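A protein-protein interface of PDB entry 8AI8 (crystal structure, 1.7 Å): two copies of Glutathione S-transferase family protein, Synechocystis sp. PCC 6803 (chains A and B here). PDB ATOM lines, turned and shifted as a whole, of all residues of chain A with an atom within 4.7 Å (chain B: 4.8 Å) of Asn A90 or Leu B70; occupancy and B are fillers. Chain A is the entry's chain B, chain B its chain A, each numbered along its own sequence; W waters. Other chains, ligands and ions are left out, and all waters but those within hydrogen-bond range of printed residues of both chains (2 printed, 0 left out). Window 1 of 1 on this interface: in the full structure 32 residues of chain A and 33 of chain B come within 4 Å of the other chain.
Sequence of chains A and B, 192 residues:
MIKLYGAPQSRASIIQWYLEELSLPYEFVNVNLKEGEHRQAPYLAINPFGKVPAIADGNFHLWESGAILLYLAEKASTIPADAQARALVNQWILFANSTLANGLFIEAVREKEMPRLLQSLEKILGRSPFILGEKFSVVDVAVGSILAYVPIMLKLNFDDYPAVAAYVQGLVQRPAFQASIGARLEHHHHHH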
ATOM      1  N   LEU A  70     -24.354  13.205 -15.877  1.00  0.00           N
ATOM      2  CA  LEU A  70     -25.023  13.896 -16.995  1.00  0.00           C
ATOM      3  C   LEU A  70     -24.567  13.374 -18.351  1.00  0.00           C
ATOM      4  O   LEU A  70     -25.388  13.233 -19.275  1.00  0.00           O
ATOM      5  CB  LEU A  70     -24.813  15.409 -16.934  1.00  0.00           C
ATOM      6  CG  LEU A  70     -25.249  16.061 -15.635  1.00  0.00           C
ATOM      7  CD1 LEU A  70     -24.670  17.476 -15.524  1.00  0.00           C
ATOM      8  CD2 LEU A  70     -26.770  16.075 -15.513  1.00  0.00           C
ATOM      9  N   ARG A  86     -32.485  19.559 -20.499  1.00  0.00           N
ATOM     10  CA  ARG A  86     -31.160  19.294 -19.926  1.00  0.00           C
ATOM     11  C   ARG A  86     -30.960  20.170 -18.683  1.00  0.00           C
ATOM     12  O   ARG A  86     -30.404  19.689 -17.700  1.00  0.00           O
ATOM     13  CB  ARG A  86     -30.042  19.617 -20.929  1.00  0.00           C
ATOM     14  CG  ARG A  86     -29.672  18.446 -21.820  1.00  0.00           C
ATOM     15  CD  ARG A  86     -28.413  18.747 -22.612  1.00  0.00           C
ATOM     16  NE  ARG A  86     -28.627  19.840 -23.563  1.00  0.00           N
ATOM     17  CZ  ARG A  86     -29.087  19.674 -24.799  1.00  0.00           C
ATOM     18  NH1 ARG A  86     -29.376  18.457 -25.251  1.00  0.00           N
ATOM     19  NH2 ARG A  86     -29.258  20.722 -25.595  1.00  0.00           N
ATOM     20  N   ALA A  87     -31.402  21.438 -18.734  1.00  0.00           N
ATOM     21  CA  ALA A  87     -31.247  22.359 -17.600  1.00  0.00           C
ATOM     22  C   ALA A  87     -31.909  21.842 -16.324  1.00  0.00           C
ATOM     23  O   ALA A  87     -31.347  22.023 -15.243  1.00  0.00           O
ATOM     24  CB  ALA A  87     -31.786  23.754 -17.941  1.00  0.00           C
ATOM     25  N   LEU A  88     -33.109  21.253 -16.428  1.00  0.00           N
ATOM     26  CA  LEU A  88     -33.781  20.747 -15.221  1.00  0.00           C
ATOM     27  C   LEU A  88     -32.999  19.582 -14.634  1.00  0.00           C
ATOM     28  O   LEU A  88     -32.889  19.479 -13.415  1.00  0.00           O
ATOM     29  CB  LEU A  88     -35.236  20.360 -15.488  1.00  0.00           C
ATOM     30  CG  LEU A  88     -36.146  21.549 -15.873  1.00  0.00           C
ATOM     31  CD1 LEU A  88     -37.562  21.071 -16.120  1.00  0.00           C
ATOM     32  CD2 LEU A  88     -36.122  22.653 -14.795  1.00  0.00           C
ATOM     33  N   VAL A  89     -32.406  18.728 -15.497  1.00  0.00           N
ATOM     34  CA  VAL A  89     -31.564  17.645 -14.975  1.00  0.00           C
ATOM     35  C   VAL A  89     -30.283  18.235 -14.337  1.00  0.00           C
ATOM     36  O   VAL A  89     -29.950  17.856 -13.217  1.00  0.00           O
ATOM     37  CB  VAL A  89     -31.250  16.572 -16.041  1.00  0.00           C
ATOM     38  CG1 VAL A  89     -30.329  15.498 -15.457  1.00  0.00           C
ATOM     39  CG2 VAL A  89     -32.548  15.931 -16.541  1.00  0.00           C
ATOM     40  N   ASN A  90     -29.627  19.195 -15.005  1.00  0.00           N
ATOM     41  CA  ASN A  90     -28.413  19.876 -14.515  1.00  0.00           C
ATOM     42  C   ASN A  90     -28.692  20.543 -13.154  1.00  0.00           C
ATOM     43  O   ASN A  90     -27.882  20.455 -12.231  1.00  0.00           O
ATOM     44  CB  ASN A  90     -27.962  20.949 -15.515  1.00  0.00           C
ATOM     45  CG  ASN A  90     -27.442  20.408 -16.825  1.00  0.00           C
ATOM     46  OD1 ASN A  90     -27.207  19.213 -16.957  1.00  0.00           O
ATOM     47  ND2 ASN A  90     -27.273  21.280 -17.836  1.00  0.00           N
ATOM     48  N   GLN A  91     -29.879  21.166 -13.014  1.00  0.00           N
ATOM     49  CA  GLN A  91     -30.294  21.806 -11.756  1.00  0.00           C
ATOM     50  C   GLN A  91     -30.198  20.824 -10.585  1.00  0.00           C
ATOM     51  O   GLN A  91     -29.564  21.123  -9.564  1.00  0.00           O
ATOM     52  CB  GLN A  91     -31.754  22.315 -11.910  1.00  0.00           C
ATOM     53  CG  GLN A  91     -32.415  22.805 -10.607  1.00  0.00           C
ATOM     54  CD  GLN A  91     -33.861  23.094 -10.922  1.00  0.00           C
ATOM     55  OE1 GLN A  91     -34.207  24.210 -11.346  1.00  0.00           O
ATOM     56  NE2 GLN A  91     -34.704  22.079 -10.787  1.00  0.00           N
ATOM     57  N   TRP A  92     -30.759  19.621 -10.770  1.00  0.00           N
ATOM     58  CA  TRP A  92     -30.773  18.642  -9.692  1.00  0.00           C
ATOM     59  C   TRP A  92     -29.396  18.053  -9.420  1.00  0.00           C
ATOM     60  O   TRP A  92     -29.094  17.727  -8.285  1.00  0.00           O
ATOM     61  CB  TRP A  92     -31.807  17.547  -9.983  1.00  0.00           C
ATOM     62  CG  TRP A  92     -33.222  18.025  -9.798  1.00  0.00           C
ATOM     63  CD1 TRP A  92     -34.128  18.345 -10.768  1.00  0.00           C
ATOM     64  CD2 TRP A  92     -33.856  18.295  -8.545  1.00  0.00           C
ATOM     65  NE1 TRP A  92     -35.311  18.777 -10.183  1.00  0.00           N
ATOM     66  CE2 TRP A  92     -35.158  18.770  -8.822  1.00  0.00           C
ATOM     67  CE3 TRP A  92     -33.427  18.239  -7.214  1.00  0.00           C
ATOM     68  CZ2 TRP A  92     -36.034  19.159  -7.805  1.00  0.00           C
ATOM     69  CZ3 TRP A  92     -34.326  18.543  -6.213  1.00  0.00           C
ATOM     70  CH2 TRP A  92     -35.606  19.021  -6.518  1.00  0.00           C
ATOM     71  N   ILE A  93     -28.574  17.917 -10.453  1.00  0.00           N
ATOM     72  CA  ILE A  93     -27.210  17.385 -10.257  1.00  0.00           C
ATOM     73  C   ILE A  93     -26.354  18.426  -9.522  1.00  0.00           C
ATOM     74  O   ILE A  93     -25.614  18.077  -8.607  1.00  0.00           O
ATOM     75  CB  ILE A  93     -26.607  16.889 -11.609  1.00  0.00           C
ATOM     76  CG1 ILE A  93     -27.018  15.429 -11.894  1.00  0.00           C
ATOM     77  CG2 ILE A  93     -25.065  16.959 -11.604  1.00  0.00           C
ATOM     78  CD1 ILE A  93     -28.499  15.076 -11.860  1.00  0.00           C
ATOM     79  N   LEU A  94     -26.505  19.718  -9.870  1.00  0.00           N
ATOM     80  CA  LEU A  94     -25.781  20.783  -9.174  1.00  0.00           C
ATOM     81  C   LEU A  94     -26.249  20.839  -7.709  1.00  0.00           C
ATOM     82  O   LEU A  94     -25.428  20.939  -6.799  1.00  0.00           O
ATOM     83  CB  LEU A  94     -25.991  22.162  -9.857  1.00  0.00           C
ATOM     84  CG  LEU A  94     -24.889  22.635 -10.817  1.00  0.00           C
ATOM     85  CD1 LEU A  94     -23.521  22.746 -10.103  1.00  0.00           C
ATOM     86  CD2 LEU A  94     -24.805  21.760 -12.036  1.00  0.00           C
ATOM     87  N   GLY B  66     -24.937  27.198 -11.101  1.00  0.00           N
ATOM     88  CA  GLY B  66     -24.230  26.427 -12.118  1.00  0.00           C
ATOM     89  C   GLY B  66     -25.120  25.995 -13.260  1.00  0.00           C
ATOM     90  O   GLY B  66     -24.720  26.066 -14.424  1.00  0.00           O
ATOM     91  N   ALA B  67     -26.355  25.552 -12.942  1.00  0.00           N
ATOM     92  CA  ALA B  67     -27.291  25.138 -13.985  1.00  0.00           C
ATOM     93  C   ALA B  67     -27.717  26.342 -14.826  1.00  0.00           C
ATOM     94  O   ALA B  67     -27.830  26.231 -16.062  1.00  0.00           O
ATOM     95  CB  ALA B  67     -28.511  24.457 -13.366  1.00  0.00           C
ATOM     96  N   ILE B  68     -27.877  27.514 -14.182  1.00  0.00           N
ATOM     97  CA  ILE B  68     -28.239  28.728 -14.903  1.00  0.00           C
ATOM     98  C   ILE B  68     -27.125  29.121 -15.870  1.00  0.00           C
ATOM     99  O   ILE B  68     -27.400  29.412 -17.030  1.00  0.00           O
ATOM    100  CB  ILE B  68     -28.525  29.871 -13.913  1.00  0.00           C
ATOM    101  CG1 ILE B  68     -29.732  29.492 -13.040  1.00  0.00           C
ATOM    102  CG2 ILE B  68     -28.805  31.178 -14.699  1.00  0.00           C
ATOM    103  CD1 ILE B  68     -29.899  30.464 -11.837  1.00  0.00           C
ATOM    104  N   LEU B  69     -25.856  29.058 -15.419  1.00  0.00           N
ATOM    105  CA  LEU B  69     -24.729  29.367 -16.318  1.00  0.00           C
ATOM    106  C   LEU B  69     -24.711  28.422 -17.525  1.00  0.00           C
ATOM    107  O   LEU B  69     -24.573  28.889 -18.660  1.00  0.00           O
ATOM    108  CB  LEU B  69     -23.374  29.309 -15.585  1.00  0.00           C
ATOM    109  CG  LEU B  69     -23.101  30.412 -14.564  1.00  0.00           C
ATOM    110  CD1 LEU B  69     -21.729  30.167 -13.864  1.00  0.00           C
ATOM    111  CD2 LEU B  69     -23.177  31.838 -15.208  1.00  0.00           C
ATOM    112  N   LEU B  70     -24.869  27.111 -17.290  1.00  0.00           N
ATOM    113  CA  LEU B  70     -24.882  26.143 -18.396  1.00  0.00           C
ATOM    114  C   LEU B  70     -26.026  26.400 -19.378  1.00  0.00           C
ATOM    115  O   LEU B  70     -25.836  26.347 -20.600  1.00  0.00           O
ATOM    116  CB  LEU B  70     -24.991  24.722 -17.819  1.00  0.00           C
ATOM    117  CG  LEU B  70     -23.788  24.319 -17.001  1.00  0.00           C
ATOM    118  CD1 LEU B  70     -24.060  23.028 -16.220  1.00  0.00           C
ATOM    119  CD2 LEU B  70     -22.566  24.155 -17.908  1.00  0.00           C
ATOM    120  N   TYR B  71     -27.206  26.720 -18.839  1.00  0.00           N
ATOM    121  CA  TYR B  71     -28.385  26.995 -19.653  1.00  0.00           C
ATOM    122  C   TYR B  71     -28.154  28.233 -20.534  1.00  0.00           C
ATOM    123  O   TYR B  71     -28.416  28.186 -21.739  1.00  0.00           O
ATOM    124  CB  TYR B  71     -29.609  27.220 -18.735  1.00  0.00           C
ATOM    125  CG  TYR B  71     -30.857  27.653 -19.484  1.00  0.00           C
ATOM    126  CD1 TYR B  71     -31.533  26.769 -20.309  1.00  0.00           C
ATOM    127  CD2 TYR B  71     -31.338  28.953 -19.387  1.00  0.00           C
ATOM    128  CE1 TYR B  71     -32.672  27.159 -21.010  1.00  0.00           C
ATOM    129  CE2 TYR B  71     -32.467  29.363 -20.096  1.00  0.00           C
ATOM    130  CZ  TYR B  71     -33.143  28.452 -20.888  1.00  0.00           C
ATOM    131  OH  TYR B  71     -34.270  28.825 -21.590  1.00  0.00           O
ATOM    132  N   LEU B  72     -27.664  29.329 -19.950  1.00  0.00           N
ATOM    133  CA  LEU B  72     -27.417  30.560 -20.716  1.00  0.00           C
ATOM    134  C   LEU B  72     -26.345  30.301 -21.790  1.00  0.00           C
ATOM    135  O   LEU B  72     -26.479  30.780 -22.921  1.00  0.00           O
ATOM    136  CB  LEU B  72     -26.969  31.668 -19.779  1.00  0.00           C
ATOM    137  CG  LEU B  72     -28.049  32.166 -18.799  1.00  0.00           C
ATOM    138  CD1 LEU B  72     -27.454  33.198 -17.842  1.00  0.00           C
ATOM    139  CD2 LEU B  72     -29.251  32.776 -19.562  1.00  0.00           C
ATOM    140  N   ALA B  73     -25.316  29.501 -21.449  1.00  0.00           N
ATOM    141  CA  ALA B  73     -24.253  29.189 -22.411  1.00  0.00           C
ATOM    142  C   ALA B  73     -24.778  28.375 -23.586  1.00  0.00           C
ATOM    143  O   ALA B  73     -24.391  28.643 -24.734  1.00  0.00           O
ATOM    144  CB  ALA B  73     -23.103  28.465 -21.716  1.00  0.00           C
ATOM    145  N   GLU B  74     -25.690  27.430 -23.322  1.00  0.00           N
ATOM    146  CA  GLU B  74     -26.293  26.597 -24.360  1.00  0.00           C
ATOM    147  C   GLU B  74     -27.143  27.471 -25.268  1.00  0.00           C
ATOM    148  O   GLU B  74     -27.027  27.392 -26.489  1.00  0.00           O
ATOM    149  CB  GLU B  74     -27.209  25.521 -23.741  1.00  0.00           C
ATOM    150  CG  GLU B  74     -26.532  24.227 -23.354  1.00  0.00           C
ATOM    151  CD  GLU B  74     -27.502  23.066 -23.448  1.00  0.00           C
ATOM    152  OE1 GLU B  74     -27.717  22.381 -22.425  1.00  0.00           O
ATOM    153  OE2 GLU B  74     -28.081  22.872 -24.540  1.00  0.00           O
ATOM    154  N   VAL B  89     -17.747  21.453 -20.281  1.00  0.00           N
ATOM    155  CA  VAL B  89     -18.205  22.663 -19.600  1.00  0.00           C
ATOM    156  C   VAL B  89     -18.903  22.268 -18.286  1.00  0.00           C
ATOM    157  O   VAL B  89     -18.651  22.895 -17.253  1.00  0.00           O
ATOM    158  CB  VAL B  89     -19.090  23.529 -20.527  1.00  0.00           C
ATOM    159  CG1 VAL B  89     -19.568  24.759 -19.782  1.00  0.00           C
ATOM    160  CG2 VAL B  89     -18.294  23.933 -21.780  1.00  0.00           C
ATOM    161  N   ASN B  90     -19.721  21.204 -18.298  1.00  0.00           N
ATOM    162  CA  ASN B  90     -20.426  20.709 -17.097  1.00  0.00           C
ATOM    163  C   ASN B  90     -19.395  20.361 -15.992  1.00  0.00           C
ATOM    164  O   ASN B  90     -19.560  20.701 -14.824  1.00  0.00           O
ATOM    165  CB  ASN B  90     -21.250  19.450 -17.446  1.00  0.00           C
ATOM    166  CG  ASN B  90     -22.442  19.691 -18.357  1.00  0.00           C
ATOM    167  OD1 ASN B  90     -22.820  20.839 -18.634  1.00  0.00           O
ATOM    168  ND2 ASN B  90     -23.076  18.616 -18.841  1.00  0.00           N
ATOM    169  N   ILE B  93     -18.130  23.518 -14.316  1.00  0.00           N
ATOM    170  CA  ILE B  93     -19.185  24.168 -13.506  1.00  0.00           C
ATOM    171  C   ILE B  93     -19.407  23.378 -12.192  1.00  0.00           C
ATOM    172  O   ILE B  93     -19.466  23.958 -11.095  1.00  0.00           O
ATOM    173  CB  ILE B  93     -20.470  24.384 -14.366  1.00  0.00           C
ATOM    174  CG1 ILE B  93     -20.417  25.733 -15.139  1.00  0.00           C
ATOM    175  CG2 ILE B  93     -21.750  24.426 -13.478  1.00  0.00           C
ATOM    176  CD1 ILE B  93     -19.198  26.053 -15.920  1.00  0.00           C
HETATM  177  O   HOH W   1     -25.855  20.943 -20.450  1.00  0.00           O
HETATM  178  O   HOH W   2     -28.406  23.903 -17.529  1.00  0.00           O
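Leu A70 touches Asn B90 (CD1 to ND2, 3.9 Å). CD1 of Tyr B71 touches CB of Ala A87 (3.8 Å). C of Asn A90 touches CB of Ala B67 (3.9 Å). Leu B70 touches Asn A90. CA of Gln A91 touches CB of Ala B67 (3.6 Å). CG of Leu A94 touches N of Ala B67 (3.9 Å).
The side-chain carboxylate (OE2) of Glu B74 is in salt-bridge range of the guanidinium group (NH2) of Arg A86.
The backbone carbonyl oxygen (O) of Arg A86 sits close to the side-chain amide oxygen (OD1) of Asn A90, at 3.3 Å. The indole nitrogen (NE1) of Trp A92 lies close to the side-chain amide nitrogen (NE2) of Gln A91.
Hydrophobic or aromatic side chains of chain B within 4 Å of the printed part of chain A: Ala B67, Leu B70 and Tyr B71. Of the 10 printed residues of chain A, 6 touch a printed residue of chain B. Among the printed residues, 7 pairs touch across the chains. Among the printed residues, Asp or Glu carboxylates within 4 Å of a Lys or Arg side-chain nitrogen of the other chain: Arg A86 with Glu B74.
Water W2 lies within hydrogen-bond range of the backbone carbonyl oxygen (O) of Ala B67 (2.8 Å), the side-chain amide nitrogen (ND2) of Asn A90 (2.9 Å) and the backbone NH (N) of Tyr B71 (3.3 Å). Water W1 bridges ND2 of Asn A90 and OE1 of Glu B74.
Leu A70 touches Asn B90, and with the chains exchanged Asn A90 touches Leu B70. Of the 7 pairs that touch across the chains among the printed residues, 2 have their exchanged pair printed and touching as well.
Val A89 touches none of the printed residues of chain B. Printed residues of chain B within 4 Å of Asn A90: Ala B67 (3.9 Å) and Leu B70 (3.999 Å). Printed residues of chain B within 4 Å of Leu A94: Ala B67. Of the printed residues of chain A, Ala B67 touches Asn A90 (3.9 Å), Gln A91 (3.6 Å) and Leu A94 (3.9 Å). Printed residues of chain A within 4 Å of Leu B70: Asn A90 (3.999 Å). Printed residues of chain A within 4 Å of Tyr B71: Ala A87 (3.8 Å). Leu B72 touches none of the printed residues of chain A.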
